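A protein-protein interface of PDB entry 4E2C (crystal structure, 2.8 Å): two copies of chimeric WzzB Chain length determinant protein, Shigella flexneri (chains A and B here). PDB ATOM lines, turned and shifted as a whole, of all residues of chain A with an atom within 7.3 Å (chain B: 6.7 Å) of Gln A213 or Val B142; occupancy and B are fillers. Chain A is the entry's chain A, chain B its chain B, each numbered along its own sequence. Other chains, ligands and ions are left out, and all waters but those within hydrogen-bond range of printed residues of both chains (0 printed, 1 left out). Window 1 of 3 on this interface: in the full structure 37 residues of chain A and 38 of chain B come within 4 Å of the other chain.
Among the printed residues, merely in contact across the chains: Tyr A209 with Gln B146 (3.2 Å), Gln A213 with Gln B139 (3.4 Å), Gln A213 with Val B142 (3.6 Å), Leu A216 with Val B141 (3.7 Å), Tyr A209 with Val B142 (3.7 Å) and Leu A216 with Thr B138 (3.8 Å).
Of the 16 printed residues of chain A, 4 touch a printed residue of chain B.
Along chain A the printed residues that touch a printed residue of chain B span positions 209 to 217.
Printed residues of chain B that touch a printed residue of chain A: Thr B138, Gln B139, Val B141, Val B142 and Gln B146.
Hydrophobic or aromatic side chains of chain B that line the printed part of chain A: Val B141 and Val B142.
Among the printed residues, 8 pairs touch across the chains.
Among the printed residues, no Asp or Glu carboxylate lies within 4 Å of a Lys or Arg side-chain nitrogen of the other chain.
Positions printed for both chains: 136 and 207.
Of the 8 pairs that touch across the chains among the printed residues, none has its exchanged pair printed and touching as well.
NE2 of Gln A213 is in hydrogen-bond range of OG1 of Thr B138.
The side-chain carboxylate of Asp A217 lies within hydrogen-bond range of the side-chain hydroxyl of Thr B138.
NE2 of Gln A213 is in hydrogen-bond range of OD2 of Asp A217 (2.8 Å).
OG1 of Thr B138 is in hydrogen-bond range of O of Ser B135 (3.2 Å).
The backbone carbonyl oxygen (O) of Asp B134 lies within hydrogen-bond range of the side-chain hydroxyl (OG1) of Thr B138, at 3.1 Å.
The side-chain amide nitrogen of Asn B207 is in hydrogen-bond range of the side-chain amide oxygen of Gln B139, at 3.2 Å.
The side-chain amide nitrogen of Gln B139 is in hydrogen-bond range of the side-chain hydroxyl of Ser B135, 2.9 Å away.
Gln A213 touches three residues of chain B.
Of the printed residues of chain A, Thr B138 touches Gln A213, Leu A216 and Asp A217.
Printed residues of chain A within 4 Å of Val B141: Leu A216 (3.7 Å).
Of the printed residues of chain A, Val B142 touches Tyr A209 (3.7 Å) and Gln A213 (3.6 Å).
Glu B145 touches none of the printed residues of chain A.
The nearest residue of chain B that does not touch Gln A213 is Ser B135 (4.4 Å).
The nearest residue of chain A that does not touch Val B142 is Leu A216 (4.2 Å).
The nearest printed residue of chain A that does not touch Gln B146 is Gln A210 (7.0 Å).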
ATOM      1  N   VAL A  33     -28.284  24.635 -18.488  1.00  0.00           N
ATOM      2  CA  VAL A  33     -26.902  24.699 -18.966  1.00  0.00           C
ATOM      3  C   VAL A  33     -26.433  26.140 -18.916  1.00  0.00           C
ATOM      4  O   VAL A  33     -25.255  26.419 -18.761  1.00  0.00           O
ATOM      5  CB  VAL A  33     -26.743  24.157 -20.402  1.00  0.00           C
ATOM      6  CG1 VAL A  33     -25.438  24.644 -21.014  1.00  0.00           C
ATOM      7  CG2 VAL A  33     -26.819  22.631 -20.427  1.00  0.00           C
ATOM      8  N   LEU A 132     -18.705  33.543 -21.172  1.00  0.00           N
ATOM      9  CA  LEU A 132     -17.904  32.441 -20.700  1.00  0.00           C
ATOM     10  C   LEU A 132     -16.474  32.585 -21.204  1.00  0.00           C
ATOM     11  O   LEU A 132     -15.525  32.598 -20.418  1.00  0.00           O
ATOM     12  CB  LEU A 132     -18.506  31.127 -21.162  1.00  0.00           C
ATOM     13  CG  LEU A 132     -19.805  30.772 -20.449  1.00  0.00           C
ATOM     14  CD1 LEU A 132     -20.316  29.431 -20.928  1.00  0.00           C
ATOM     15  CD2 LEU A 132     -19.597  30.742 -18.951  1.00  0.00           C
ATOM     16  N   LEU A 136     -12.978  33.191 -19.079  1.00  0.00           N
ATOM     17  CA  LEU A 136     -11.794  32.348 -19.133  1.00  0.00           C
ATOM     18  C   LEU A 136     -10.531  33.170 -19.265  1.00  0.00           C
ATOM     19  O   LEU A 136      -9.533  32.890 -18.596  1.00  0.00           O
ATOM     20  CB  LEU A 136     -11.869  31.352 -20.278  1.00  0.00           C
ATOM     21  CG  LEU A 136     -12.799  30.159 -20.083  1.00  0.00           C
ATOM     22  CD1 LEU A 136     -12.589  29.196 -21.224  1.00  0.00           C
ATOM     23  CD2 LEU A 136     -12.541  29.465 -18.763  1.00  0.00           C
ATOM     24  N   ASN A 207     -12.930  26.070 -10.408  1.00  0.00           N
ATOM     25  CA  ASN A 207     -13.847  27.043 -10.969  1.00  0.00           C
ATOM     26  C   ASN A 207     -13.501  27.278 -12.428  1.00  0.00           C
ATOM     27  O   ASN A 207     -14.370  27.441 -13.276  1.00  0.00           O
ATOM     28  CB  ASN A 207     -13.825  28.363 -10.186  1.00  0.00           C
ATOM     29  CG  ASN A 207     -14.838  29.367 -10.718  1.00  0.00           C
ATOM     30  OD1 ASN A 207     -16.039  29.132 -10.655  1.00  0.00           O
ATOM     31  ND2 ASN A 207     -14.357  30.479 -11.263  1.00  0.00           N
ATOM     32  N   TYR A 208     -12.217  27.306 -12.728  1.00  0.00           N
ATOM     33  CA  TYR A 208     -11.825  27.494 -14.109  1.00  0.00           C
ATOM     34  C   TYR A 208     -12.337  26.343 -14.985  1.00  0.00           C
ATOM     35  O   TYR A 208     -12.697  26.555 -16.145  1.00  0.00           O
ATOM     36  CB  TYR A 208     -10.316  27.622 -14.218  1.00  0.00           C
ATOM     37  CG  TYR A 208      -9.818  27.734 -15.630  1.00  0.00           C
ATOM     38  CD1 TYR A 208      -9.575  28.965 -16.194  1.00  0.00           C
ATOM     39  CD2 TYR A 208      -9.575  26.603 -16.396  1.00  0.00           C
ATOM     40  CE1 TYR A 208      -9.115  29.081 -17.491  1.00  0.00           C
ATOM     41  CE2 TYR A 208      -9.099  26.701 -17.696  1.00  0.00           C
ATOM     42  CZ  TYR A 208      -8.876  27.950 -18.237  1.00  0.00           C
ATOM     43  OH  TYR A 208      -8.408  28.084 -19.525  1.00  0.00           O
ATOM     44  N   TYR A 209     -12.375  25.132 -14.435  1.00  0.00           N
ATOM     45  CA  TYR A 209     -12.881  23.992 -15.193  1.00  0.00           C
ATOM     46  C   TYR A 209     -14.396  23.962 -15.241  1.00  0.00           C
ATOM     47  O   TYR A 209     -14.971  23.449 -16.196  1.00  0.00           O
ATOM     48  CB  TYR A 209     -12.324  22.677 -14.649  1.00  0.00           C
ATOM     49  CG  TYR A 209     -10.853  22.603 -14.895  1.00  0.00           C
ATOM     50  CD1 TYR A 209     -10.373  22.452 -16.179  1.00  0.00           C
ATOM     51  CD2 TYR A 209      -9.935  22.739 -13.855  1.00  0.00           C
ATOM     52  CE1 TYR A 209      -9.026  22.413 -16.434  1.00  0.00           C
ATOM     53  CE2 TYR A 209      -8.581  22.700 -14.099  1.00  0.00           C
ATOM     54  CZ  TYR A 209      -8.134  22.538 -15.397  1.00  0.00           C
ATOM     55  OH  TYR A 209      -6.796  22.490 -15.681  1.00  0.00           O
ATOM     56  N   GLN A 210     -15.044  24.496 -14.207  1.00  0.00           N
ATOM     57  CA  GLN A 210     -16.493  24.605 -14.237  1.00  0.00           C
ATOM     58  C   GLN A 210     -16.865  25.464 -15.427  1.00  0.00           C
ATOM     59  O   GLN A 210     -17.758  25.121 -16.197  1.00  0.00           O
ATOM     60  CB  GLN A 210     -17.035  25.224 -12.953  1.00  0.00           C
ATOM     61  CG  GLN A 210     -18.170  24.420 -12.319  1.00  0.00           C
ATOM     62  CD  GLN A 210     -18.965  23.632 -13.338  1.00  0.00           C
ATOM     63  OE1 GLN A 210     -19.566  24.196 -14.247  1.00  0.00           O
ATOM     64  NE2 GLN A 210     -18.947  22.314 -13.205  1.00  0.00           N
ATOM     65  N   THR A 211     -16.145  26.570 -15.588  1.00  0.00           N
ATOM     66  CA  THR A 211     -16.387  27.483 -16.693  1.00  0.00           C
ATOM     67  C   THR A 211     -16.203  26.751 -18.015  1.00  0.00           C
ATOM     68  O   THR A 211     -17.136  26.697 -18.814  1.00  0.00           O
ATOM     69  CB  THR A 211     -15.507  28.760 -16.607  1.00  0.00           C
ATOM     70  OG1 THR A 211     -15.898  29.531 -15.469  1.00  0.00           O
ATOM     71  CG2 THR A 211     -15.689  29.635 -17.821  1.00  0.00           C
ATOM     72  N   LYS A 212     -15.028  26.164 -18.243  1.00  0.00           N
ATOM     73  CA  LYS A 212     -14.801  25.408 -19.480  1.00  0.00           C
ATOM     74  C   LYS A 212     -15.936  24.405 -19.724  1.00  0.00           C
ATOM     75  O   LYS A 212     -16.462  24.296 -20.838  1.00  0.00           O
ATOM     76  CB  LYS A 212     -13.441  24.692 -19.485  1.00  0.00           C
ATOM     77  N   GLN A 213     -16.329  23.688 -18.677  1.00  0.00           N
ATOM     78  CA  GLN A 213     -17.420  22.735 -18.791  1.00  0.00           C
ATOM     79  C   GLN A 213     -18.659  23.427 -19.328  1.00  0.00           C
ATOM     80  O   GLN A 213     -19.251  22.973 -20.306  1.00  0.00           O
ATOM     81  CB  GLN A 213     -17.743  22.118 -17.437  1.00  0.00           C
ATOM     82  CG  GLN A 213     -18.912  21.167 -17.479  1.00  0.00           C
ATOM     83  CD  GLN A 213     -18.594  19.887 -18.227  1.00  0.00           C
ATOM     84  OE1 GLN A 213     -17.524  19.309 -18.050  1.00  0.00           O
ATOM     85  NE2 GLN A 213     -19.521  19.439 -19.067  1.00  0.00           N
ATOM     86  N   THR A 214     -19.047  24.534 -18.692  1.00  0.00           N
ATOM     87  CA  THR A 214     -20.300  25.199 -19.058  1.00  0.00           C
ATOM     88  C   THR A 214     -20.277  25.691 -20.493  1.00  0.00           C
ATOM     89  O   THR A 214     -21.284  25.676 -21.175  1.00  0.00           O
ATOM     90  CB  THR A 214     -20.623  26.357 -18.119  1.00  0.00           C
ATOM     91  OG1 THR A 214     -20.947  25.831 -16.832  1.00  0.00           O
ATOM     92  CG2 THR A 214     -21.811  27.139 -18.632  1.00  0.00           C
ATOM     93  N   LEU A 215     -19.106  26.099 -20.957  1.00  0.00           N
ATOM     94  CA  LEU A 215     -18.961  26.605 -22.312  1.00  0.00           C
ATOM     95  C   LEU A 215     -19.140  25.493 -23.332  1.00  0.00           C
ATOM     96  O   LEU A 215     -19.672  25.711 -24.421  1.00  0.00           O
ATOM     97  CB  LEU A 215     -17.584  27.231 -22.478  1.00  0.00           C
ATOM     98  CG  LEU A 215     -17.336  27.902 -23.823  1.00  0.00           C
ATOM     99  CD1 LEU A 215     -18.422  28.926 -24.089  1.00  0.00           C
ATOM    100  CD2 LEU A 215     -15.976  28.555 -23.824  1.00  0.00           C
ATOM    101  N   LEU A 216     -18.693  24.297 -22.973  1.00  0.00           N
ATOM    102  CA  LEU A 216     -18.760  23.170 -23.884  1.00  0.00           C
ATOM    103  C   LEU A 216     -20.196  22.717 -24.015  1.00  0.00           C
ATOM    104  O   LEU A 216     -20.623  22.277 -25.080  1.00  0.00           O
ATOM    105  CB  LEU A 216     -17.887  22.021 -23.391  1.00  0.00           C
ATOM    106  CG  LEU A 216     -16.382  22.258 -23.528  1.00  0.00           C
ATOM    107  CD1 LEU A 216     -15.580  21.117 -22.910  1.00  0.00           C
ATOM    108  CD2 LEU A 216     -16.039  22.432 -24.987  1.00  0.00           C
ATOM    109  N   ASP A 217     -20.938  22.835 -22.924  1.00  0.00           N
ATOM    110  CA  ASP A 217     -22.333  22.459 -22.930  1.00  0.00           C
ATOM    111  C   ASP A 217     -23.199  23.528 -23.586  1.00  0.00           C
ATOM    112  O   ASP A 217     -24.128  23.205 -24.326  1.00  0.00           O
ATOM    113  CB  ASP A 217     -22.785  22.122 -21.517  1.00  0.00           C
ATOM    114  CG  ASP A 217     -22.248  20.770 -21.061  1.00  0.00           C
ATOM    115  OD1 ASP A 217     -22.165  19.857 -21.928  1.00  0.00           O
ATOM    116  OD2 ASP A 217     -21.902  20.621 -19.855  1.00  0.00           O
ATOM    117  N   ILE A 218     -22.874  24.797 -23.343  1.00  0.00           N
ATOM    118  CA  ILE A 218     -23.475  25.887 -24.116  1.00  0.00           C
ATOM    119  C   ILE A 218     -23.287  25.673 -25.621  1.00  0.00           C
ATOM    120  O   ILE A 218     -24.227  25.829 -26.385  1.00  0.00           O
ATOM    121  CB  ILE A 218     -22.932  27.289 -23.733  1.00  0.00           C
ATOM    122  N   LYS A 219     -22.083  25.305 -26.045  1.00  0.00           N
ATOM    123  CA  LYS A 219     -21.822  25.158 -27.472  1.00  0.00           C
ATOM    124  C   LYS A 219     -22.616  23.990 -28.039  1.00  0.00           C
ATOM    125  O   LYS A 219     -23.075  24.029 -29.173  1.00  0.00           O
ATOM    126  CB  LYS A 219     -20.325  24.967 -27.750  1.00  0.00           C
ATOM    127  CG  LYS A 219     -19.486  26.221 -27.585  1.00  0.00           C
ATOM    128  CD  LYS A 219     -18.024  25.990 -27.998  1.00  0.00           C
ATOM    129  N   ASP B 134     -24.145  13.258 -23.416  1.00  0.00           N
ATOM    130  CA  ASP B 134     -23.440  14.483 -23.798  1.00  0.00           C
ATOM    131  C   ASP B 134     -22.644  15.081 -22.628  1.00  0.00           C
ATOM    132  O   ASP B 134     -21.520  15.582 -22.794  1.00  0.00           O
ATOM    133  CB  ASP B 134     -24.439  15.507 -24.351  1.00  0.00           C
ATOM    134  CG  ASP B 134     -24.817  15.241 -25.811  1.00  0.00           C
ATOM    135  OD1 ASP B 134     -24.834  14.067 -26.241  1.00  0.00           O
ATOM    136  OD2 ASP B 134     -25.094  16.221 -26.539  1.00  0.00           O
ATOM    137  N   SER B 135     -23.227  15.015 -21.439  1.00  0.00           N
ATOM    138  CA  SER B 135     -22.529  15.470 -20.271  1.00  0.00           C
ATOM    139  C   SER B 135     -21.254  14.638 -20.117  1.00  0.00           C
ATOM    140  O   SER B 135     -20.179  15.167 -19.852  1.00  0.00           O
ATOM    141  CB  SER B 135     -23.402  15.312 -19.043  1.00  0.00           C
ATOM    142  OG  SER B 135     -23.034  16.248 -18.050  1.00  0.00           O
ATOM    143  N   LEU B 136     -21.371  13.330 -20.301  1.00  0.00           N
ATOM    144  CA  LEU B 136     -20.224  12.458 -20.159  1.00  0.00           C
ATOM    145  C   LEU B 136     -19.146  12.849 -21.157  1.00  0.00           C
ATOM    146  O   LEU B 136     -17.951  12.875 -20.828  1.00  0.00           O
ATOM    147  CB  LEU B 136     -20.627  11.007 -20.346  1.00  0.00           C
ATOM    148  CG  LEU B 136     -21.425  10.375 -19.209  1.00  0.00           C
ATOM    149  CD1 LEU B 136     -21.628   8.881 -19.480  1.00  0.00           C
ATOM    150  CD2 LEU B 136     -20.744  10.578 -17.865  1.00  0.00           C
ATOM    151  N   ARG B 137     -19.582  13.182 -22.368  1.00  0.00           N
ATOM    152  CA  ARG B 137     -18.658  13.460 -23.449  1.00  0.00           C
ATOM    153  C   ARG B 137     -17.861  14.726 -23.154  1.00  0.00           C
ATOM    154  O   ARG B 137     -16.625  14.738 -23.280  1.00  0.00           O
ATOM    155  CB  ARG B 137     -19.421  13.620 -24.749  1.00  0.00           C
ATOM    156  CG  ARG B 137     -18.577  13.592 -26.010  1.00  0.00           C
ATOM    157  CD  ARG B 137     -19.408  13.947 -27.256  1.00  0.00           C
ATOM    158  NE  ARG B 137     -19.389  15.382 -27.547  1.00  0.00           N
ATOM    159  CZ  ARG B 137     -20.475  16.134 -27.709  1.00  0.00           C
ATOM    160  NH1 ARG B 137     -21.689  15.595 -27.608  1.00  0.00           N
ATOM    161  NH2 ARG B 137     -20.345  17.435 -27.973  1.00  0.00           N
ATOM    162  N   THR B 138     -18.567  15.789 -22.768  1.00  0.00           N
ATOM    163  CA  THR B 138     -17.908  17.073 -22.546  1.00  0.00           C
ATOM    164  C   THR B 138     -17.059  17.045 -21.288  1.00  0.00           C
ATOM    165  O   THR B 138     -16.038  17.715 -21.207  1.00  0.00           O
ATOM    166  CB  THR B 138     -18.898  18.256 -22.446  1.00  0.00           C
ATOM    167  OG1 THR B 138     -19.952  17.920 -21.539  1.00  0.00           O
ATOM    168  CG2 THR B 138     -19.461  18.624 -23.821  1.00  0.00           C
ATOM    169  N   GLN B 139     -17.496  16.280 -20.298  1.00  0.00           N
ATOM    170  CA  GLN B 139     -16.720  16.120 -19.079  1.00  0.00           C
ATOM    171  C   GLN B 139     -15.393  15.422 -19.400  1.00  0.00           C
ATOM    172  O   GLN B 139     -14.379  15.685 -18.771  1.00  0.00           O
ATOM    173  CB  GLN B 139     -17.515  15.338 -18.021  1.00  0.00           C
ATOM    174  CG  GLN B 139     -18.612  16.147 -17.377  1.00  0.00           C
ATOM    175  CD  GLN B 139     -19.423  15.344 -16.387  1.00  0.00           C
ATOM    176  OE1 GLN B 139     -18.881  14.764 -15.449  1.00  0.00           O
ATOM    177  NE2 GLN B 139     -20.733  15.298 -16.595  1.00  0.00           N
ATOM    178  N   GLU B 140     -15.404  14.542 -20.391  1.00  0.00           N
ATOM    179  CA  GLU B 140     -14.183  13.869 -20.763  1.00  0.00           C
ATOM    180  C   GLU B 140     -13.223  14.843 -21.436  1.00  0.00           C
ATOM    181  O   GLU B 140     -12.007  14.748 -21.254  1.00  0.00           O
ATOM    182  CB  GLU B 140     -14.457  12.647 -21.628  1.00  0.00           C
ATOM    183  CG  GLU B 140     -13.178  11.987 -22.127  1.00  0.00           C
ATOM    184  CD  GLU B 140     -13.376  10.552 -22.588  1.00  0.00           C
ATOM    185  OE1 GLU B 140     -14.445   9.976 -22.281  1.00  0.00           O
ATOM    186  OE2 GLU B 140     -12.462  10.007 -23.258  1.00  0.00           O
ATOM    187  N   VAL B 141     -13.766  15.800 -22.182  1.00  0.00           N
ATOM    188  CA  VAL B 141     -12.934  16.803 -22.849  1.00  0.00           C
ATOM    189  C   VAL B 141     -12.165  17.601 -21.797  1.00  0.00           C
ATOM    190  O   VAL B 141     -10.989  17.924 -21.978  1.00  0.00           O
ATOM    191  CB  VAL B 141     -13.774  17.741 -23.775  1.00  0.00           C
ATOM    192  CG1 VAL B 141     -12.954  18.938 -24.257  1.00  0.00           C
ATOM    193  CG2 VAL B 141     -14.330  16.967 -24.965  1.00  0.00           C
ATOM    194  N   VAL B 142     -12.824  17.893 -20.680  1.00  0.00           N
ATOM    195  CA  VAL B 142     -12.185  18.619 -19.592  1.00  0.00           C
ATOM    196  C   VAL B 142     -11.114  17.783 -18.905  1.00  0.00           C
ATOM    197  O   VAL B 142     -10.018  18.266 -18.598  1.00  0.00           O
ATOM    198  CB  VAL B 142     -13.230  19.044 -18.539  1.00  0.00           C
ATOM    199  CG1 VAL B 142     -12.546  19.619 -17.289  1.00  0.00           C
ATOM    200  CG2 VAL B 142     -14.185  20.047 -19.142  1.00  0.00           C
ATOM    201  N   ALA B 143     -11.456  16.526 -18.644  1.00  0.00           N
ATOM    202  CA  ALA B 143     -10.593  15.615 -17.906  1.00  0.00           C
ATOM    203  C   ALA B 143      -9.348  15.372 -18.764  1.00  0.00           C
ATOM    204  O   ALA B 143      -8.233  15.230 -18.280  1.00  0.00           O
ATOM    205  CB  ALA B 143     -11.344  14.323 -17.649  1.00  0.00           C
ATOM    206  N   GLN B 144      -9.572  15.384 -20.067  1.00  0.00           N
ATOM    207  CA  GLN B 144      -8.530  15.218 -21.033  1.00  0.00           C
ATOM    208  C   GLN B 144      -7.636  16.408 -20.979  1.00  0.00           C
ATOM    209  O   GLN B 144      -6.426  16.304 -21.193  1.00  0.00           O
ATOM    210  CB  GLN B 144      -9.139  15.153 -22.404  1.00  0.00           C
ATOM    211  CG  GLN B 144      -8.113  15.083 -23.462  1.00  0.00           C
ATOM    212  CD  GLN B 144      -7.393  13.781 -23.392  1.00  0.00           C
ATOM    213  OE1 GLN B 144      -8.024  12.723 -23.267  1.00  0.00           O
ATOM    214  NE2 GLN B 144      -6.056  13.835 -23.436  1.00  0.00           N
ATOM    215  N   GLU B 145      -8.209  17.570 -20.710  1.00  0.00           N
ATOM    216  CA  GLU B 145      -7.359  18.750 -20.631  1.00  0.00           C
ATOM    217  C   GLU B 145      -6.510  18.666 -19.396  1.00  0.00           C
ATOM    218  O   GLU B 145      -5.344  19.020 -19.434  1.00  0.00           O
ATOM    219  CB  GLU B 145      -8.148  20.045 -20.682  1.00  0.00           C
ATOM    220  CG  GLU B 145      -8.749  20.254 -22.054  1.00  0.00           C
ATOM    221  CD  GLU B 145      -9.398  21.610 -22.223  1.00  0.00           C
ATOM    222  OE1 GLU B 145     -10.112  22.047 -21.292  1.00  0.00           O
ATOM    223  OE2 GLU B 145      -9.188  22.231 -23.293  1.00  0.00           O
ATOM    224  N   GLN B 146      -7.095  18.163 -18.315  1.00  0.00           N
ATOM    225  CA  GLN B 146      -6.370  18.033 -17.065  1.00  0.00           C
ATOM    226  C   GLN B 146      -5.172  17.090 -17.192  1.00  0.00           C
ATOM    227  O   GLN B 146      -4.083  17.390 -16.684  1.00  0.00           O
ATOM    228  CB  GLN B 146      -7.329  17.659 -15.936  1.00  0.00           C
ATOM    229  CG  GLN B 146      -8.195  18.869 -15.591  1.00  0.00           C
ATOM    230  CD  GLN B 146      -9.457  18.553 -14.819  1.00  0.00           C
ATOM    231  OE1 GLN B 146      -9.951  17.421 -14.807  1.00  0.00           O
ATOM    232  NE2 GLN B 146     -10.004  19.569 -14.184  1.00  0.00           N
ATOM    233  N   LYS B 147      -5.363  15.976 -17.898  1.00  0.00           N
ATOM    234  CA  LYS B 147      -4.279  15.052 -18.111  1.00  0.00           C
ATOM    235  C   LYS B 147      -3.184  15.734 -18.909  1.00  0.00           C
ATOM    236  O   LYS B 147      -2.000  15.564 -18.617  1.00  0.00           O
ATOM    237  CB  LYS B 147      -4.733  13.809 -18.871  1.00  0.00           C
ATOM    238  CG  LYS B 147      -3.555  12.903 -19.172  1.00  0.00           C
ATOM    239  CD  LYS B 147      -3.871  11.806 -20.151  1.00  0.00           C
ATOM    240  CE  LYS B 147      -2.817  11.734 -21.256  1.00  0.00           C
ATOM    241  N   LEU B 202      -7.208   8.764 -18.037  1.00  0.00           N
ATOM    242  CA  LEU B 202      -7.766   9.980 -17.459  1.00  0.00           C
ATOM    243  C   LEU B 202      -8.286   9.728 -16.034  1.00  0.00           C
ATOM    244  O   LEU B 202      -8.828   8.656 -15.739  1.00  0.00           O
ATOM    245  CB  LEU B 202      -8.898  10.515 -18.333  1.00  0.00           C
ATOM    246  CG  LEU B 202      -8.557  10.785 -19.791  1.00  0.00           C
ATOM    247  CD1 LEU B 202      -9.644  11.607 -20.413  1.00  0.00           C
ATOM    248  CD2 LEU B 202      -7.242  11.513 -19.886  1.00  0.00           C
ATOM    249  N   ASN B 207     -18.271  13.717  -9.850  1.00  0.00           N
ATOM    250  CA  ASN B 207     -19.424  14.199 -10.623  1.00  0.00           C
ATOM    251  C   ASN B 207     -19.563  13.416 -11.902  1.00  0.00           C
ATOM    252  O   ASN B 207     -20.661  13.144 -12.362  1.00  0.00           O
ATOM    253  CB  ASN B 207     -19.336  15.708 -10.944  1.00  0.00           C
ATOM    254  CG  ASN B 207     -20.501  16.196 -11.808  1.00  0.00           C
ATOM    255  OD1 ASN B 207     -21.631  16.314 -11.339  1.00  0.00           O
ATOM    256  ND2 ASN B 207     -20.226  16.476 -13.076  1.00  0.00           N
